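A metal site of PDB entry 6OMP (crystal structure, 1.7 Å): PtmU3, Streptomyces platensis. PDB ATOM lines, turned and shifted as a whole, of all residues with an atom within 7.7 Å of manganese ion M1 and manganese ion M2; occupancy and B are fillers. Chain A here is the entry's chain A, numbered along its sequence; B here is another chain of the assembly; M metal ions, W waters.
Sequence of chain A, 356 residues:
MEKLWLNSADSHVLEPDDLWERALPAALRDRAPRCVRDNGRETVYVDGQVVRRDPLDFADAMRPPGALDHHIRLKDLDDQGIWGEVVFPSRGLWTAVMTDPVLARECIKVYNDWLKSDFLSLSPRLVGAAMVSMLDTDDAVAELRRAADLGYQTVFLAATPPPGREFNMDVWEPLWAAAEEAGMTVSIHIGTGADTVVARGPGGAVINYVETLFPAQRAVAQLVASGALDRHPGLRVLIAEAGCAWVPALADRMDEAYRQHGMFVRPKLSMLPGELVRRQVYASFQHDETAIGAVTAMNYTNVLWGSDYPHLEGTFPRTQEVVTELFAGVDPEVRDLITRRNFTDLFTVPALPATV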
ATOM      1  N   ALA A   9     -10.624  -6.260 -11.334  1.00  0.00           N
ATOM      2  CA  ALA A   9      -9.509  -6.292 -10.350  1.00  0.00           C
ATOM      3  C   ALA A   9      -9.023  -4.902  -9.915  1.00  0.00           C
ATOM      4  O   ALA A   9      -8.052  -4.840  -9.157  1.00  0.00           O
ATOM      5  CB  ALA A   9      -8.350  -7.067 -10.913  1.00  0.00           C
ATOM      6  N   ASP A  10      -9.680  -3.816 -10.296  1.00  0.00           N
ATOM      7  CA  ASP A  10      -9.187  -2.466  -9.997  1.00  0.00           C
ATOM      8  C   ASP A  10     -10.296  -1.416 -10.106  1.00  0.00           C
ATOM      9  O   ASP A  10     -10.948  -1.270 -11.133  1.00  0.00           O
ATOM     10  CB  ASP A  10      -8.017  -2.159 -10.940  1.00  0.00           C
ATOM     11  CG  ASP A  10      -7.408  -0.781 -10.753  1.00  0.00           C
ATOM     12  OD1 ASP A  10      -7.602  -0.192  -9.696  1.00  0.00           O
ATOM     13  OD2 ASP A  10      -6.714  -0.337 -11.711  1.00  0.00           O
ATOM     14  N   SER A  11     -10.415  -0.678  -9.030  1.00  0.00           N
ATOM     15  CA  SER A  11     -11.209   0.570  -8.941  1.00  0.00           C
ATOM     16  C   SER A  11     -10.783   1.316  -7.704  1.00  0.00           C
ATOM     17  O   SER A  11     -10.092   0.706  -6.859  1.00  0.00           O
ATOM     18  CB  SER A  11     -12.705   0.296  -8.945  1.00  0.00           C
ATOM     19  OG  SER A  11     -13.120  -0.246  -7.714  1.00  0.00           O
ATOM     20  N   HIS A  12     -11.332   2.523  -7.562  1.00  0.00           N
ATOM     21  CA  HIS A  12     -10.982   3.412  -6.434  1.00  0.00           C
ATOM     22  C   HIS A  12     -12.262   3.934  -5.776  1.00  0.00           C
ATOM     23  O   HIS A  12     -13.250   4.219  -6.491  1.00  0.00           O
ATOM     24  CB  HIS A  12     -10.061   4.559  -6.852  1.00  0.00           C
ATOM     25  CG  HIS A  12      -8.825   4.020  -7.463  1.00  0.00           C
ATOM     26  ND1 HIS A  12      -7.661   3.835  -6.741  1.00  0.00           N
ATOM     27  CD2 HIS A  12      -8.608   3.511  -8.701  1.00  0.00           C
ATOM     28  CE1 HIS A  12      -6.777   3.232  -7.539  1.00  0.00           C
ATOM     29  NE2 HIS A  12      -7.335   3.009  -8.715  1.00  0.00           N
ATOM     30  N   VAL A  86     -12.653  -5.143  -7.008  1.00  0.00           N
ATOM     31  CA  VAL A  86     -11.658  -4.749  -6.002  1.00  0.00           C
ATOM     32  C   VAL A  86     -11.675  -3.255  -5.882  1.00  0.00           C
ATOM     33  O   VAL A  86     -11.846  -2.560  -6.913  1.00  0.00           O
ATOM     34  CB  VAL A  86     -10.262  -5.292  -6.368  1.00  0.00           C
ATOM     35  CG1 VAL A  86      -9.187  -4.816  -5.403  1.00  0.00           C
ATOM     36  CG2 VAL A  86     -10.280  -6.799  -6.462  1.00  0.00           C
ATOM     37  N   PHE A  88      -9.610   0.007  -4.325  1.00  0.00           N
ATOM     38  CA  PHE A  88      -8.393   0.611  -3.766  1.00  0.00           C
ATOM     39  C   PHE A  88      -8.710   1.974  -3.174  1.00  0.00           C
ATOM     40  O   PHE A  88      -9.694   2.618  -3.539  1.00  0.00           O
ATOM     41  CB  PHE A  88      -7.316   0.722  -4.858  1.00  0.00           C
ATOM     42  CG  PHE A  88      -6.730  -0.606  -5.238  1.00  0.00           C
ATOM     43  CD1 PHE A  88      -5.804  -1.239  -4.421  1.00  0.00           C
ATOM     44  CD2 PHE A  88      -7.098  -1.220  -6.423  1.00  0.00           C
ATOM     45  CE1 PHE A  88      -5.287  -2.476  -4.789  1.00  0.00           C
ATOM     46  CE2 PHE A  88      -6.560  -2.440  -6.807  1.00  0.00           C
ATOM     47  CZ  PHE A  88      -5.652  -3.069  -5.997  1.00  0.00           C
ATOM     48  N   PRO A  89      -7.827   2.512  -2.298  1.00  0.00           N
ATOM     49  CA  PRO A  89      -8.009   3.876  -1.801  1.00  0.00           C
ATOM     50  C   PRO A  89      -7.829   4.933  -2.879  1.00  0.00           C
ATOM     51  O   PRO A  89      -7.357   4.608  -3.969  1.00  0.00           O
ATOM     52  CB  PRO A  89      -6.911   4.018  -0.743  1.00  0.00           C
ATOM     53  CG  PRO A  89      -6.399   2.647  -0.460  1.00  0.00           C
ATOM     54  CD  PRO A  89      -6.655   1.843  -1.722  1.00  0.00           C
ATOM     55  N   LEU A  93      -4.010   6.568  -0.426  1.00  0.00           N
ATOM     56  CA  LEU A  93      -2.776   6.131  -1.108  1.00  0.00           C
ATOM     57  C   LEU A  93      -1.630   7.044  -0.679  1.00  0.00           C
ATOM     58  O   LEU A  93      -0.489   6.576  -0.728  1.00  0.00           O
ATOM     59  CB  LEU A  93      -2.941   6.221  -2.620  1.00  0.00           C
ATOM     60  CG  LEU A  93      -4.026   5.342  -3.249  1.00  0.00           C
ATOM     61  CD1 LEU A  93      -4.150   5.620  -4.743  1.00  0.00           C
ATOM     62  CD2 LEU A  93      -3.786   3.896  -2.964  1.00  0.00           C
ATOM     63  N   HIS A 189      -0.285  -1.403  -6.261  1.00  0.00           N
ATOM     64  CA  HIS A 189      -0.971  -0.533  -7.235  1.00  0.00           C
ATOM     65  C   HIS A 189       0.045   0.488  -7.728  1.00  0.00           C
ATOM     66  O   HIS A 189       0.737   1.141  -6.908  1.00  0.00           O
ATOM     67  CB  HIS A 189      -2.258   0.100  -6.688  1.00  0.00           C
ATOM     68  CG  HIS A 189      -3.024   0.779  -7.754  1.00  0.00           C
ATOM     69  ND1 HIS A 189      -2.576   1.930  -8.370  1.00  0.00           N
ATOM     70  CD2 HIS A 189      -4.263   0.546  -8.236  1.00  0.00           C
ATOM     71  CE1 HIS A 189      -3.424   2.295  -9.284  1.00  0.00           C
ATOM     72  NE2 HIS A 189      -4.500   1.476  -9.223  1.00  0.00           N
ATOM     73  N   ILE A 190       0.105   0.684  -9.036  1.00  0.00           N
ATOM     74  CA  ILE A 190       1.121   1.646  -9.539  1.00  0.00           C
ATOM     75  C   ILE A 190       0.743   3.088  -9.225  1.00  0.00           C
ATOM     76  O   ILE A 190      -0.414   3.424  -8.784  1.00  0.00           O
ATOM     77  CB  ILE A 190       1.471   1.445 -11.037  1.00  0.00           C
ATOM     78  CG1 ILE A 190       0.301   1.417 -12.004  1.00  0.00           C
ATOM     79  CG2 ILE A 190       2.336   0.200 -11.169  1.00  0.00           C
ATOM     80  CD1 ILE A 190      -0.520   2.642 -12.089  1.00  0.00           C
ATOM     81  N   TYR A 209       2.760   8.668 -18.066  1.00  0.00           N
ATOM     82  CA  TYR A 209       1.903   7.472 -17.996  1.00  0.00           C
ATOM     83  C   TYR A 209       2.785   6.238 -18.138  1.00  0.00           C
ATOM     84  O   TYR A 209       2.531   5.249 -17.432  1.00  0.00           O
ATOM     85  CB  TYR A 209       0.740   7.538 -18.977  1.00  0.00           C
ATOM     86  CG  TYR A 209      -0.355   6.573 -18.645  1.00  0.00           C
ATOM     87  CD1 TYR A 209      -1.034   6.645 -17.438  1.00  0.00           C
ATOM     88  CD2 TYR A 209      -0.725   5.559 -19.513  1.00  0.00           C
ATOM     89  CE1 TYR A 209      -2.026   5.741 -17.106  1.00  0.00           C
ATOM     90  CE2 TYR A 209      -1.763   4.674 -19.221  1.00  0.00           C
ATOM     91  CZ  TYR A 209      -2.435   4.781 -18.008  1.00  0.00           C
ATOM     92  OH  TYR A 209      -3.423   3.891 -17.675  1.00  0.00           O
ATOM     93  N   ALA A 240      -1.516  -3.973  -9.940  1.00  0.00           N
ATOM     94  CA  ALA A 240      -2.723  -3.280 -10.440  1.00  0.00           C
ATOM     95  C   ALA A 240      -2.400  -2.047 -11.281  1.00  0.00           C
ATOM     96  O   ALA A 240      -1.656  -1.147 -10.812  1.00  0.00           O
ATOM     97  CB  ALA A 240      -3.607  -2.965  -9.254  1.00  0.00           C
ATOM     98  N   GLU A 241      -2.977  -1.994 -12.483  1.00  0.00           N
ATOM     99  CA  GLU A 241      -3.117  -0.803 -13.348  1.00  0.00           C
ATOM    100  C   GLU A 241      -1.798  -0.533 -14.099  1.00  0.00           C
ATOM    101  O   GLU A 241      -1.580   0.613 -14.547  1.00  0.00           O
ATOM    102  CB  GLU A 241      -3.542   0.428 -12.556  1.00  0.00           C
ATOM    103  CG  GLU A 241      -4.329   1.383 -13.438  1.00  0.00           C
ATOM    104  CD  GLU A 241      -4.667   2.729 -12.859  1.00  0.00           C
ATOM    105  OE1 GLU A 241      -5.219   2.791 -11.705  1.00  0.00           O
ATOM    106  OE2 GLU A 241      -4.506   3.764 -13.580  1.00  0.00           O
ATOM    107  N   ALA A 242      -1.071  -1.589 -14.350  1.00  0.00           N
ATOM    108  CA  ALA A 242       0.227  -1.474 -15.093  1.00  0.00           C
ATOM    109  C   ALA A 242       0.133  -2.145 -16.462  1.00  0.00           C
ATOM    110  O   ALA A 242       1.139  -2.145 -17.176  1.00  0.00           O
ATOM    111  CB  ALA A 242       1.311  -2.002 -14.186  1.00  0.00           C
ATOM    112  N   SER A 284      -3.254  -6.523 -13.837  1.00  0.00           N
ATOM    113  CA  SER A 284      -4.526  -6.032 -14.356  1.00  0.00           C
ATOM    114  C   SER A 284      -4.305  -5.038 -15.496  1.00  0.00           C
ATOM    115  O   SER A 284      -3.194  -4.382 -15.612  1.00  0.00           O
ATOM    116  CB  SER A 284      -5.340  -5.503 -13.211  1.00  0.00           C
ATOM    117  OG  SER A 284      -4.971  -4.164 -12.879  1.00  0.00           O
ATOM    118  N   GLN A 286      -7.014  -2.347 -18.413  1.00  0.00           N
ATOM    119  CA  GLN A 286      -8.359  -1.807 -18.706  1.00  0.00           C
ATOM    120  C   GLN A 286      -8.621  -1.991 -20.204  1.00  0.00           C
ATOM    121  O   GLN A 286      -9.651  -2.598 -20.561  1.00  0.00           O
ATOM    122  CB  GLN A 286      -8.555  -0.374 -18.214  1.00  0.00           C
ATOM    123  CG  GLN A 286      -8.205  -0.162 -16.726  1.00  0.00           C
ATOM    124  CD  GLN A 286      -6.762   0.264 -16.567  1.00  0.00           C
ATOM    125  OE1 GLN A 286      -5.982  -0.435 -15.930  1.00  0.00           O
ATOM    126  NE2 GLN A 286      -6.428   1.438 -17.097  1.00  0.00           N
ATOM    127  N   SER A 307     -11.695  -2.311 -14.368  1.00  0.00           N
ATOM    128  CA  SER A 307     -12.387  -1.144 -14.921  1.00  0.00           C
ATOM    129  C   SER A 307     -11.629   0.145 -14.635  1.00  0.00           C
ATOM    130  O   SER A 307     -11.852   1.088 -15.362  1.00  0.00           O
ATOM    131  CB  SER A 307     -13.780  -0.981 -14.381  1.00  0.00           C
ATOM    132  OG  SER A 307     -13.762  -0.437 -13.072  1.00  0.00           O
ATOM    133  N   ASP A 308     -10.891   0.167 -13.549  1.00  0.00           N
ATOM    134  CA  ASP A 308     -10.263   1.353 -12.930  1.00  0.00           C
ATOM    135  C   ASP A 308     -11.255   2.492 -12.765  1.00  0.00           C
ATOM    136  O   ASP A 308     -10.884   3.645 -12.769  1.00  0.00           O
ATOM    137  CB  ASP A 308      -9.002   1.857 -13.663  1.00  0.00           C
ATOM    138  CG  ASP A 308      -8.133   2.728 -12.787  1.00  0.00           C
ATOM    139  OD1 ASP A 308      -7.892   2.404 -11.578  1.00  0.00           O
ATOM    140  OD2 ASP A 308      -7.512   3.645 -13.349  1.00  0.00           O
ATOM    141  N   TYR A 309     -12.521   2.161 -12.487  1.00  0.00           N
ATOM    142  CA  TYR A 309     -13.489   3.186 -12.084  1.00  0.00           C
ATOM    143  C   TYR A 309     -12.993   3.957 -10.870  1.00  0.00           C
ATOM    144  O   TYR A 309     -12.529   3.370  -9.904  1.00  0.00           O
ATOM    145  CB  TYR A 309     -14.787   2.470 -11.689  1.00  0.00           C
ATOM    146  CG  TYR A 309     -15.969   3.366 -11.388  1.00  0.00           C
ATOM    147  CD1 TYR A 309     -16.145   3.865 -10.120  1.00  0.00           C
ATOM    148  CD2 TYR A 309     -16.878   3.717 -12.382  1.00  0.00           C
ATOM    149  CE1 TYR A 309     -17.269   4.637  -9.793  1.00  0.00           C
ATOM    150  CE2 TYR A 309     -18.018   4.449 -12.072  1.00  0.00           C
ATOM    151  CZ  TYR A 309     -18.159   4.968 -10.794  1.00  0.00           C
ATOM    152  OH  TYR A 309     -19.308   5.637 -10.443  1.00  0.00           O
ATOM    153  N   PRO A 310     -13.192   5.293 -10.783  1.00  0.00           N
ATOM    154  CA  PRO A 310     -13.724   6.153 -11.822  1.00  0.00           C
ATOM    155  C   PRO A 310     -12.703   7.011 -12.554  1.00  0.00           C
ATOM    156  O   PRO A 310     -13.055   8.105 -13.040  1.00  0.00           O
ATOM    157  CB  PRO A 310     -14.532   7.147 -10.991  1.00  0.00           C
ATOM    158  CG  PRO A 310     -13.778   7.297  -9.746  1.00  0.00           C
ATOM    159  CD  PRO A 310     -13.021   6.017  -9.528  1.00  0.00           C
ATOM    160  N   HIS A 311     -11.498   6.475 -12.702  1.00  0.00           N
ATOM    161  CA  HIS A 311     -10.371   7.218 -13.325  1.00  0.00           C
ATOM    162  C   HIS A 311     -10.628   7.406 -14.849  1.00  0.00           C
ATOM    163  O   HIS A 311     -11.213   6.515 -15.527  1.00  0.00           O
ATOM    164  CB  HIS A 311      -9.053   6.539 -12.968  1.00  0.00           C
ATOM    165  CG  HIS A 311      -8.655   6.585 -11.544  1.00  0.00           C
ATOM    166  ND1 HIS A 311      -7.535   5.914 -11.092  1.00  0.00           N
ATOM    167  CD2 HIS A 311      -9.203   7.171 -10.454  1.00  0.00           C
ATOM    168  CE1 HIS A 311      -7.395   6.127  -9.806  1.00  0.00           C
ATOM    169  NE2 HIS A 311      -8.424   6.868  -9.375  1.00  0.00           N
ATOM    170  N   LEU A 312      -9.997   8.445 -15.413  1.00  0.00           N
ATOM    171  CA  LEU A 312     -10.022   8.712 -16.855  1.00  0.00           C
ATOM    172  C   LEU A 312      -9.512   7.481 -17.610  1.00  0.00           C
ATOM    173  O   LEU A 312     -10.067   7.208 -18.653  1.00  0.00           O
ATOM    174  CB  LEU A 312      -9.147   9.931 -17.192  1.00  0.00           C
ATOM    175  CG  LEU A 312      -9.660  11.299 -16.745  1.00  0.00           C
ATOM    176  CD1 LEU A 312      -8.678  12.366 -17.202  1.00  0.00           C
ATOM    177  CD2 LEU A 312     -11.029  11.580 -17.353  1.00  0.00           C
ATOM    178  N   GLU A 313      -8.502   6.781 -17.089  1.00  0.00           N
ATOM    179  CA  GLU A 313      -7.822   5.682 -17.826  1.00  0.00           C
ATOM    180  C   GLU A 313      -8.637   4.388 -17.702  1.00  0.00           C
ATOM    181  O   GLU A 313      -8.295   3.362 -18.311  1.00  0.00           O
ATOM    182  CB  GLU A 313      -6.380   5.519 -17.362  1.00  0.00           C
ATOM    183  CG  GLU A 313      -6.210   5.288 -15.872  1.00  0.00           C
ATOM    184  CD  GLU A 313      -6.081   6.531 -14.998  1.00  0.00           C
ATOM    185  OE1 GLU A 313      -6.335   7.637 -15.473  1.00  0.00           O
ATOM    186  OE2 GLU A 313      -5.823   6.370 -13.808  1.00  0.00           O
ATOM    187  N   GLY A 314      -9.728   4.453 -16.949  1.00  0.00           N
ATOM    188  CA  GLY A 314     -10.638   3.300 -16.887  1.00  0.00           C
ATOM    189  C   GLY A 314     -11.608   3.264 -18.039  1.00  0.00           C
ATOM    190  O   GLY A 314     -11.550   4.134 -18.916  1.00  0.00           O
ATOM    191  N   ARG B 253       0.129   1.029 -23.660  1.00  0.00           N
ATOM    192  CA  ARG B 253       0.192   1.969 -22.524  1.00  0.00           C
ATOM    193  C   ARG B 253       0.068   3.391 -23.104  1.00  0.00           C
ATOM    194  O   ARG B 253      -0.689   4.217 -22.578  1.00  0.00           O
ATOM    195  CB  ARG B 253       1.493   1.794 -21.724  1.00  0.00           C
ATOM    196  CG  ARG B 253       1.619   2.660 -20.484  1.00  0.00           C
ATOM    197  CD  ARG B 253       0.744   2.103 -19.383  1.00  0.00           C
ATOM    198  NE  ARG B 253       0.904   2.728 -18.077  1.00  0.00           N
ATOM    199  CZ  ARG B 253       0.087   2.432 -17.072  1.00  0.00           C
ATOM    200  NH1 ARG B 253      -0.808   1.478 -17.235  1.00  0.00           N
ATOM    201  NH2 ARG B 253       0.251   3.026 -15.912  1.00  0.00           N
ATOM    202  N   HIS B 261      -6.431  10.417 -21.792  1.00  0.00           N
ATOM    203  CA  HIS B 261      -5.877  11.636 -21.188  1.00  0.00           C
ATOM    204  C   HIS B 261      -5.649  12.717 -22.259  1.00  0.00           C
ATOM    205  O   HIS B 261      -4.825  13.654 -21.976  1.00  0.00           O
ATOM    206  CB  HIS B 261      -4.557  11.398 -20.451  1.00  0.00           C
ATOM    207  CG  HIS B 261      -4.633  10.454 -19.310  1.00  0.00           C
ATOM    208  ND1 HIS B 261      -3.515   9.974 -18.696  1.00  0.00           N
ATOM    209  CD2 HIS B 261      -5.691   9.926 -18.668  1.00  0.00           C
ATOM    210  CE1 HIS B 261      -3.857   9.185 -17.709  1.00  0.00           C
ATOM    211  NE2 HIS B 261      -5.211   9.116 -17.690  1.00  0.00           N
HETATM  212 MN    MN M   1      -6.540   1.663 -10.360  1.00  0.00          MN
HETATM  213 MN    MN M   2      -6.005   4.842 -12.346  1.00  0.00          MN
HETATM  214  O   HOH W   1      -4.408   5.617 -10.932  1.00  0.00           O
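The side-chain carboxylate (OE1) of Glu 313 lies within hydrogen-bond range of a ring nitrogen (NE2) of His 261 of chain B, at 2.9 Å.
NE2 of Gln 286 sits at hydrogen-bond distance from O of Glu 313 (2.9 Å).
ND1 of His 12 lies within hydrogen-bond range of O of Pro 89, 2.9 Å away.
The backbone carbonyl oxygen (O) of Glu 241 is in hydrogen-bond range of the guanidinium group (NH1) of Arg 253 of chain B (2.9 Å).
N of Ser 307 sits at hydrogen-bond distance from O of Asp 10.
The backbone carbonyl oxygen (O) of Tyr 309 is in hydrogen-bond range of the backbone NH (N) of His 12, 2.8 Å away.
The side-chain hydroxyl (OG) of Ser 284 is in hydrogen-bond range of the backbone NH (N) of Glu 241, 3.0 Å away.
Within 4 Å of manganese ion M1: Asp 10, His 12, His 189, Glu 241 and Asp 308.
The nearest printed residue that does not touch manganese ion M1 is His 311 (4.4 Å).
The nearest printed residue that does not touch manganese ion M2 is His 12 (4.3 Å).
Manganese ion M1 is bound by the side-chain carboxylate (OD1) of Asp 308, the side-chain carboxylate (OE1) of Glu 241, the side-chain carboxylate (OD1) of Asp 10, a ring nitrogen (NE2) of His 12, a ring nitrogen (NE2) of His 189 and the side-chain carboxylate (OD2) of Asp 10.
Manganese ion M2 is bound by OE2 of Glu 313 (2.1 Å), OD2 of Asp 308 (2.2 Å), OE2 of Glu 241 (2.2 Å), ND1 of His 311 (2.3 Å), water W1 (2.3 Å) and OE1 of Glu 241 (2.3 Å).
Manganese ion M2 has six donor atoms within binding distance.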
